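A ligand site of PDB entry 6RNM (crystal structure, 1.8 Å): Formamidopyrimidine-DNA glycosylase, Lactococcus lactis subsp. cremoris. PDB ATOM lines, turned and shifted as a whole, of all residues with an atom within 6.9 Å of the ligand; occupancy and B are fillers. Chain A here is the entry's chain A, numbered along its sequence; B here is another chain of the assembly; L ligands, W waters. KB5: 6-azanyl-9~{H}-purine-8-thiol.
Residues that only touch the ligand: DT 10 of chain B (3.2 Å), Glu 162 (3.8 Å) and Gln 163 (3.9 Å).
A nitrogen (N3) of the ligand lies close to the backbone carbonyl oxygen (O) of Leu 161 (3.4 Å).
A nitrogen (N) of the ligand lies within hydrogen-bond range of O5' of DT 9 of chain B (3.4 Å).
The guanidinium group of Arg 260 lies close to a sulfur (S) of the ligand (3.4 Å).
NZ of Lys 57 lies close to S of the ligand.
OP2 of DT 8 of chain B sits close to S of the ligand, at 3.3 Å.
Water W3 bridges a nitrogen (N3) of the ligand and the guanidinium group (NH1) of Arg 260.
Water W2 lies within hydrogen-bond range of a nitrogen (N) of the ligand and OP2 of DT 10 of chain B.
Water W1 lies within hydrogen-bond range of O of Pro 158 and N2 of the ligand.
OP2 of DT 9 of chain B lies within salt-bridge range of the side-chain amino group (NZ) of Lys 57.
OP2 of 3DR 7 of chain B is in salt-bridge range of the guanidinium group of Arg 260 (3.0 Å).
NZ of Lys 57 lies close to NE2 of Gln 163 (3.4 Å).
NZ of Lys 57 lies within salt-bridge range of OP1 of DT 8 of chain B, 2.7 Å away.
O of Leu 161 lies within hydrogen-bond range of NE2 of Gln 163 (3.0 Å).
OP2 of DT 8 of chain B lies within salt-bridge range of the guanidinium group of Arg 260 (2.9 Å).
NE2 of Gln 163 sits at hydrogen-bond distance from O of Leu 169 (2.9 Å).
O of Leu 169 lies within hydrogen-bond range of NZ of Lys 57, at 2.8 Å.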
ATOM      1  N   GLU A   2     -12.675   7.379  -8.296  1.00  0.00           N
ATOM      2  CA  GLU A   2     -12.416   8.826  -8.399  1.00  0.00           C
ATOM      3  C   GLU A   2     -13.467   9.512  -7.508  1.00  0.00           C
ATOM      4  O   GLU A   2     -14.220   8.813  -6.835  1.00  0.00           O
ATOM      5  CB  GLU A   2     -12.464   9.306  -9.873  1.00  0.00           C
ATOM      6  CG  GLU A   2     -11.372   8.581 -10.661  1.00  0.00           C
ATOM      7  CD  GLU A   2     -11.444   8.791 -12.156  1.00  0.00           C
ATOM      8  OE1 GLU A   2     -11.587   9.960 -12.591  1.00  0.00           O
ATOM      9  OE2 GLU A   2     -11.186   7.814 -12.895  1.00  0.00           O
ATOM     10  N   LYS A  57     -10.756  12.507  -3.061  1.00  0.00           N
ATOM     11  CA  LYS A  57     -11.000  11.058  -3.191  1.00  0.00           C
ATOM     12  C   LYS A  57     -10.889  10.347  -1.806  1.00  0.00           C
ATOM     13  O   LYS A  57     -10.949   9.108  -1.739  1.00  0.00           O
ATOM     14  CB  LYS A  57      -9.995  10.422  -4.194  1.00  0.00           C
ATOM     15  CG  LYS A  57     -10.077  10.983  -5.628  1.00  0.00           C
ATOM     16  CD  LYS A  57      -8.940  10.457  -6.508  1.00  0.00           C
ATOM     17  CE  LYS A  57      -8.806  11.327  -7.750  1.00  0.00           C
ATOM     18  NZ  LYS A  57      -7.559  11.010  -8.552  1.00  0.00           N
ATOM     19  N   TYR A  58     -10.760  11.133  -0.726  1.00  0.00           N
ATOM     20  CA  TYR A  58     -10.643  10.571   0.622  1.00  0.00           C
ATOM     21  C   TYR A  58     -11.995  10.438   1.299  1.00  0.00           C
ATOM     22  O   TYR A  58     -12.750  11.416   1.384  1.00  0.00           O
ATOM     23  CB  TYR A  58      -9.742  11.449   1.516  1.00  0.00           C
ATOM     24  CG  TYR A  58      -8.298  11.542   1.084  1.00  0.00           C
ATOM     25  CD1 TYR A  58      -7.930  12.332  -0.009  1.00  0.00           C
ATOM     26  CD2 TYR A  58      -7.287  10.938   1.835  1.00  0.00           C
ATOM     27  CE1 TYR A  58      -6.596  12.447  -0.395  1.00  0.00           C
ATOM     28  CE2 TYR A  58      -5.944  11.073   1.466  1.00  0.00           C
ATOM     29  CZ  TYR A  58      -5.612  11.843   0.370  1.00  0.00           C
ATOM     30  OH  TYR A  58      -4.315  11.948  -0.043  1.00  0.00           O
ATOM     31  N   MET A  75      -6.528   2.456  -6.130  1.00  0.00           N
ATOM     32  CA  MET A  75      -6.930   1.951  -7.440  1.00  0.00           C
ATOM     33  C   MET A  75      -8.103   0.982  -7.463  1.00  0.00           C
ATOM     34  O   MET A  75      -8.859   0.962  -8.445  1.00  0.00           O
ATOM     35  CB  MET A  75      -5.734   1.295  -8.159  1.00  0.00           C
ATOM     36  CG  MET A  75      -4.639   2.292  -8.570  1.00  0.00           C
ATOM     37  SD  MET A  75      -5.258   3.480  -9.817  1.00  0.00           S
ATOM     38  CE  MET A  75      -5.239   2.440 -11.255  1.00  0.00           C
ATOM     39  N   ILE A 131      -4.205  19.450  -1.060  1.00  0.00           N
ATOM     40  CA  ILE A 131      -5.409  19.156  -1.856  1.00  0.00           C
ATOM     41  C   ILE A 131      -6.082  20.460  -2.253  1.00  0.00           C
ATOM     42  O   ILE A 131      -6.245  21.347  -1.416  1.00  0.00           O
ATOM     43  CB  ILE A 131      -6.377  18.210  -1.071  1.00  0.00           C
ATOM     44  CG1 ILE A 131      -5.691  16.877  -0.669  1.00  0.00           C
ATOM     45  CG2 ILE A 131      -7.670  17.917  -1.865  1.00  0.00           C
ATOM     46  CD1 ILE A 131      -4.931  16.082  -1.815  1.00  0.00           C
ATOM     47  N   PRO A 158      -1.682  15.900 -16.771  1.00  0.00           N
ATOM     48  CA  PRO A 158      -0.992  15.592 -15.494  1.00  0.00           C
ATOM     49  C   PRO A 158      -1.173  16.691 -14.457  1.00  0.00           C
ATOM     50  O   PRO A 158      -1.276  16.360 -13.277  1.00  0.00           O
ATOM     51  CB  PRO A 158       0.487  15.436 -15.876  1.00  0.00           C
ATOM     52  CG  PRO A 158       0.611  15.915 -17.281  1.00  0.00           C
ATOM     53  CD  PRO A 158      -0.736  15.893 -17.924  1.00  0.00           C
ATOM     54  N   LEU A 160      -3.849  18.589 -13.954  1.00  0.00           N
ATOM     55  CA  LEU A 160      -5.176  18.356 -13.335  1.00  0.00           C
ATOM     56  C   LEU A 160      -5.170  17.132 -12.423  1.00  0.00           C
ATOM     57  O   LEU A 160      -5.827  17.135 -11.386  1.00  0.00           O
ATOM     58  CB  LEU A 160      -6.253  18.149 -14.410  1.00  0.00           C
ATOM     59  CG  LEU A 160      -6.680  19.448 -15.137  1.00  0.00           C
ATOM     60  CD1 LEU A 160      -7.568  19.108 -16.344  1.00  0.00           C
ATOM     61  CD2 LEU A 160      -7.454  20.391 -14.198  1.00  0.00           C
ATOM     62  N   LEU A 161      -4.430  16.092 -12.816  1.00  0.00           N
ATOM     63  CA  LEU A 161      -4.354  14.877 -12.008  1.00  0.00           C
ATOM     64  C   LEU A 161      -3.618  15.069 -10.678  1.00  0.00           C
ATOM     65  O   LEU A 161      -3.797  14.237  -9.784  1.00  0.00           O
ATOM     66  CB  LEU A 161      -3.718  13.746 -12.819  1.00  0.00           C
ATOM     67  CG  LEU A 161      -4.629  13.147 -13.912  1.00  0.00           C
ATOM     68  CD1 LEU A 161      -3.876  12.074 -14.715  1.00  0.00           C
ATOM     69  CD2 LEU A 161      -5.897  12.522 -13.299  1.00  0.00           C
ATOM     70  N   GLU A 162      -2.819  16.153 -10.531  1.00  0.00           N
ATOM     71  CA  GLU A 162      -2.075  16.395  -9.272  1.00  0.00           C
ATOM     72  C   GLU A 162      -2.954  16.701  -8.063  1.00  0.00           C
ATOM     73  O   GLU A 162      -2.443  16.674  -6.943  1.00  0.00           O
ATOM     74  CB  GLU A 162      -1.007  17.483  -9.478  1.00  0.00           C
ATOM     75  CG  GLU A 162       0.166  16.927 -10.264  1.00  0.00           C
ATOM     76  CD  GLU A 162       1.178  17.894 -10.879  1.00  0.00           C
ATOM     77  OE1 GLU A 162       1.158  19.086 -10.511  1.00  0.00           O
ATOM     78  OE2 GLU A 162       1.981  17.460 -11.733  1.00  0.00           O
ATOM     79  N   GLN A 163      -4.260  16.982  -8.266  1.00  0.00           N
ATOM     80  CA  GLN A 163      -5.263  17.268  -7.208  1.00  0.00           C
ATOM     81  C   GLN A 163      -5.089  18.641  -6.580  1.00  0.00           C
ATOM     82  O   GLN A 163      -5.825  18.934  -5.637  1.00  0.00           O
ATOM     83  CB  GLN A 163      -5.203  16.226  -6.043  1.00  0.00           C
ATOM     84  CG  GLN A 163      -5.317  14.744  -6.466  1.00  0.00           C
ATOM     85  CD  GLN A 163      -6.595  14.520  -7.211  1.00  0.00           C
ATOM     86  OE1 GLN A 163      -7.691  14.585  -6.633  1.00  0.00           O
ATOM     87  NE2 GLN A 163      -6.454  14.181  -8.477  1.00  0.00           N
ATOM     88  N   LEU A 169     -10.386  14.598  -9.754  1.00  0.00           N
ATOM     89  CA  LEU A 169     -10.272  13.978 -11.084  1.00  0.00           C
ATOM     90  C   LEU A 169      -9.262  12.849 -11.041  1.00  0.00           C
ATOM     91  O   LEU A 169      -8.192  12.983 -10.435  1.00  0.00           O
ATOM     92  CB  LEU A 169      -9.780  15.007 -12.140  1.00  0.00           C
ATOM     93  CG  LEU A 169     -10.725  16.174 -12.407  1.00  0.00           C
ATOM     94  CD1 LEU A 169      -9.987  17.282 -13.118  1.00  0.00           C
ATOM     95  CD2 LEU A 169     -11.963  15.689 -13.241  1.00  0.00           C
ATOM     96  N   GLY A 170      -9.594  11.767 -11.723  1.00  0.00           N
ATOM     97  CA  GLY A 170      -8.704  10.648 -11.933  1.00  0.00           C
ATOM     98  C   GLY A 170      -8.638  10.387 -13.408  1.00  0.00           C
ATOM     99  O   GLY A 170      -9.083  11.236 -14.182  1.00  0.00           O
ATOM    100  N   ASN A 171      -8.117   9.229 -13.810  1.00  0.00           N
ATOM    101  CA  ASN A 171      -7.911   8.988 -15.234  1.00  0.00           C
ATOM    102  C   ASN A 171      -9.183   9.034 -16.062  1.00  0.00           C
ATOM    103  O   ASN A 171      -9.153   9.566 -17.171  1.00  0.00           O
ATOM    104  CB  ASN A 171      -7.144   7.689 -15.482  1.00  0.00           C
ATOM    105  CG  ASN A 171      -6.266   7.792 -16.725  1.00  0.00           C
ATOM    106  OD1 ASN A 171      -5.646   8.835 -16.968  1.00  0.00           O
ATOM    107  ND2 ASN A 171      -6.116   6.696 -17.453  1.00  0.00           N
ATOM    108  N   ARG A 260       0.263   7.663 -18.053  1.00  0.00           N
ATOM    109  CA  ARG A 260      -1.158   7.256 -18.004  1.00  0.00           C
ATOM    110  C   ARG A 260      -1.765   7.022 -19.389  1.00  0.00           C
ATOM    111  O   ARG A 260      -1.497   7.814 -20.306  1.00  0.00           O
ATOM    112  CB  ARG A 260      -2.006   8.319 -17.275  1.00  0.00           C
ATOM    113  CG  ARG A 260      -1.509   8.684 -15.866  1.00  0.00           C
ATOM    114  CD  ARG A 260      -1.422   7.470 -14.929  1.00  0.00           C
ATOM    115  NE  ARG A 260      -2.726   6.863 -14.647  1.00  0.00           N
ATOM    116  CZ  ARG A 260      -3.554   7.298 -13.691  1.00  0.00           C
ATOM    117  NH1 ARG A 260      -3.247   8.370 -12.973  1.00  0.00           N
ATOM    118  NH2 ARG A 260      -4.693   6.650 -13.460  1.00  0.00           N
ATOM    119  O5' 3DR B   7      -7.262   4.350 -13.951  1.00  0.00           O
ATOM    120  P   3DR B   7      -6.453   3.734 -15.201  1.00  0.00           P
ATOM    121  OP1 3DR B   7      -6.946   4.090 -16.534  1.00  0.00           O
ATOM    122  OP2 3DR B   7      -4.966   4.132 -15.014  1.00  0.00           O
ATOM    123  C2' 3DR B   7      -9.295   4.083 -10.387  1.00  0.00           C
ATOM    124  C5' 3DR B   7      -8.547   4.055 -13.578  1.00  0.00           C
ATOM    125  C4' 3DR B   7      -9.110   5.137 -12.602  1.00  0.00           C
ATOM    126  O4' 3DR B   7     -10.452   4.730 -12.379  1.00  0.00           O
ATOM    127  C1' 3DR B   7     -10.670   4.302 -11.027  1.00  0.00           C
ATOM    128  C3' 3DR B   7      -8.464   5.120 -11.157  1.00  0.00           C
ATOM    129  O3' 3DR B   7      -8.645   6.446 -10.604  1.00  0.00           O
ATOM    130  P    DT B   8      -7.448   7.456 -10.426  1.00  0.00           P
ATOM    131  OP1  DT B   8      -8.031   8.616  -9.710  1.00  0.00           O
ATOM    132  OP2  DT B   8      -6.744   7.661 -11.726  1.00  0.00           O
ATOM    133  O5'  DT B   8      -6.497   6.694  -9.397  1.00  0.00           O
ATOM    134  C5'  DT B   8      -7.023   6.368  -8.077  1.00  0.00           C
ATOM    135  C4'  DT B   8      -6.034   6.736  -7.002  1.00  0.00           C
ATOM    136  O4'  DT B   8      -4.898   5.835  -7.047  1.00  0.00           O
ATOM    137  C3'  DT B   8      -5.494   8.161  -7.081  1.00  0.00           C
ATOM    138  O3'  DT B   8      -5.708   8.801  -5.812  1.00  0.00           O
ATOM    139  C2'  DT B   8      -4.002   7.995  -7.414  1.00  0.00           C
ATOM    140  C1'  DT B   8      -3.700   6.565  -6.948  1.00  0.00           C
ATOM    141  N1   DT B   8      -2.690   5.840  -7.784  1.00  0.00           N
ATOM    142  C2   DT B   8      -1.727   5.045  -7.166  1.00  0.00           C
ATOM    143  O2   DT B   8      -1.581   4.982  -5.947  1.00  0.00           O
ATOM    144  N3   DT B   8      -0.918   4.342  -8.023  1.00  0.00           N
ATOM    145  C4   DT B   8      -0.991   4.303  -9.403  1.00  0.00           C
ATOM    146  O4   DT B   8      -0.215   3.581 -10.040  1.00  0.00           O
ATOM    147  C5   DT B   8      -2.043   5.109  -9.998  1.00  0.00           C
ATOM    148  C7   DT B   8      -2.220   5.120 -11.494  1.00  0.00           C
ATOM    149  C6   DT B   8      -2.843   5.822  -9.169  1.00  0.00           C
ATOM    150  P    DT B   9      -5.269  10.339  -5.525  1.00  0.00           P
ATOM    151  OP1  DT B   9      -6.112  10.865  -4.403  1.00  0.00           O
ATOM    152  OP2  DT B   9      -5.217  11.070  -6.791  1.00  0.00           O
ATOM    153  O5'  DT B   9      -3.800  10.169  -4.967  1.00  0.00           O
ATOM    154  C5'  DT B   9      -3.651   9.456  -3.725  1.00  0.00           C
ATOM    155  C4'  DT B   9      -2.215   9.115  -3.465  1.00  0.00           C
ATOM    156  O4'  DT B   9      -1.683   8.342  -4.550  1.00  0.00           O
ATOM    157  C3'  DT B   9      -1.271  10.308  -3.258  1.00  0.00           C
ATOM    158  O3'  DT B   9      -0.850  10.243  -1.922  1.00  0.00           O
ATOM    159  C2'  DT B   9      -0.120  10.040  -4.270  1.00  0.00           C
ATOM    160  C1'  DT B   9      -0.303   8.550  -4.566  1.00  0.00           C
ATOM    161  N1   DT B   9       0.215   8.086  -5.903  1.00  0.00           N
ATOM    162  C2   DT B   9       1.198   7.096  -5.937  1.00  0.00           C
ATOM    163  O2   DT B   9       1.745   6.648  -4.935  1.00  0.00           O
ATOM    164  N3   DT B   9       1.539   6.674  -7.204  1.00  0.00           N
ATOM    165  C4   DT B   9       1.013   7.121  -8.408  1.00  0.00           C
ATOM    166  O4   DT B   9       1.418   6.640  -9.461  1.00  0.00           O
ATOM    167  C5   DT B   9      -0.014   8.151  -8.306  1.00  0.00           C
ATOM    168  C7   DT B   9      -0.661   8.689  -9.549  1.00  0.00           C
ATOM    169  C6   DT B   9      -0.383   8.543  -7.070  1.00  0.00           C
ATOM    170  P    DT B  10       0.033  11.370  -1.199  1.00  0.00           P
ATOM    171  OP1  DT B  10      -0.225  11.262   0.263  1.00  0.00           O
ATOM    172  OP2  DT B  10      -0.130  12.666  -1.894  1.00  0.00           O
ATOM    173  O5'  DT B  10       1.514  10.874  -1.480  1.00  0.00           O
ATOM    174  C5'  DT B  10       1.999   9.683  -0.862  1.00  0.00           C
ATOM    175  C4'  DT B  10       3.413   9.417  -1.322  1.00  0.00           C
ATOM    176  O4'  DT B  10       3.363   8.948  -2.692  1.00  0.00           O
ATOM    177  C3'  DT B  10       4.328  10.659  -1.325  1.00  0.00           C
ATOM    178  O3'  DT B  10       5.508  10.413  -0.562  1.00  0.00           O
ATOM    179  C2'  DT B  10       4.649  10.876  -2.798  1.00  0.00           C
ATOM    180  C1'  DT B  10       4.481   9.474  -3.350  1.00  0.00           C
ATOM    181  N1   DT B  10       4.237   9.426  -4.800  1.00  0.00           N
ATOM    182  C2   DT B  10       4.897   8.475  -5.568  1.00  0.00           C
ATOM    183  O2   DT B  10       5.693   7.680  -5.099  1.00  0.00           O
ATOM    184  N3   DT B  10       4.602   8.518  -6.901  1.00  0.00           N
ATOM    185  C4   DT B  10       3.711   9.382  -7.534  1.00  0.00           C
ATOM    186  O4   DT B  10       3.555   9.305  -8.748  1.00  0.00           O
ATOM    187  C5   DT B  10       3.075  10.354  -6.678  1.00  0.00           C
ATOM    188  C7   DT B  10       2.119  11.359  -7.244  1.00  0.00           C
ATOM    189  C6   DT B  10       3.348  10.310  -5.366  1.00  0.00           C
HETATM  190  C4  KB5 L   1      -2.210  11.990  -8.597  1.00  0.00           C
HETATM  191  N3  KB5 L   1      -2.460  11.298 -10.718  1.00  0.00           N
HETATM  192  C2  KB5 L   1      -1.592  11.996  -9.907  1.00  0.00           C
HETATM  193  N1  KB5 L   1      -0.367  13.338  -7.898  1.00  0.00           N
HETATM  194  S   KB5 L   1      -4.821  10.011 -10.484  1.00  0.00           S
HETATM  195  C3  KB5 L   1      -3.543  10.914  -9.886  1.00  0.00           C
HETATM  196  N4  KB5 L   1      -3.424  11.311  -8.620  1.00  0.00           N
HETATM  197  C   KB5 L   1      -1.541  12.671  -7.582  1.00  0.00           C
HETATM  198  N   KB5 L   1      -2.006  12.674  -6.283  1.00  0.00           N
HETATM  199  N2  KB5 L   1      -0.424  12.612 -10.254  1.00  0.00           N
HETATM  200  C1  KB5 L   1       0.098  13.265  -9.196  1.00  0.00           C
HETATM  201  O   HOH W   1      -0.035  13.962 -12.777  1.00  0.00           O
HETATM  202  O   HOH W   2      -2.111  14.002  -3.799  1.00  0.00           O
HETATM  203  O   HOH W   3      -1.118  10.300 -12.930  1.00  0.00           O
HETATM  204  O   HOH W   4       1.200  14.745  -6.122  1.00  0.00           O
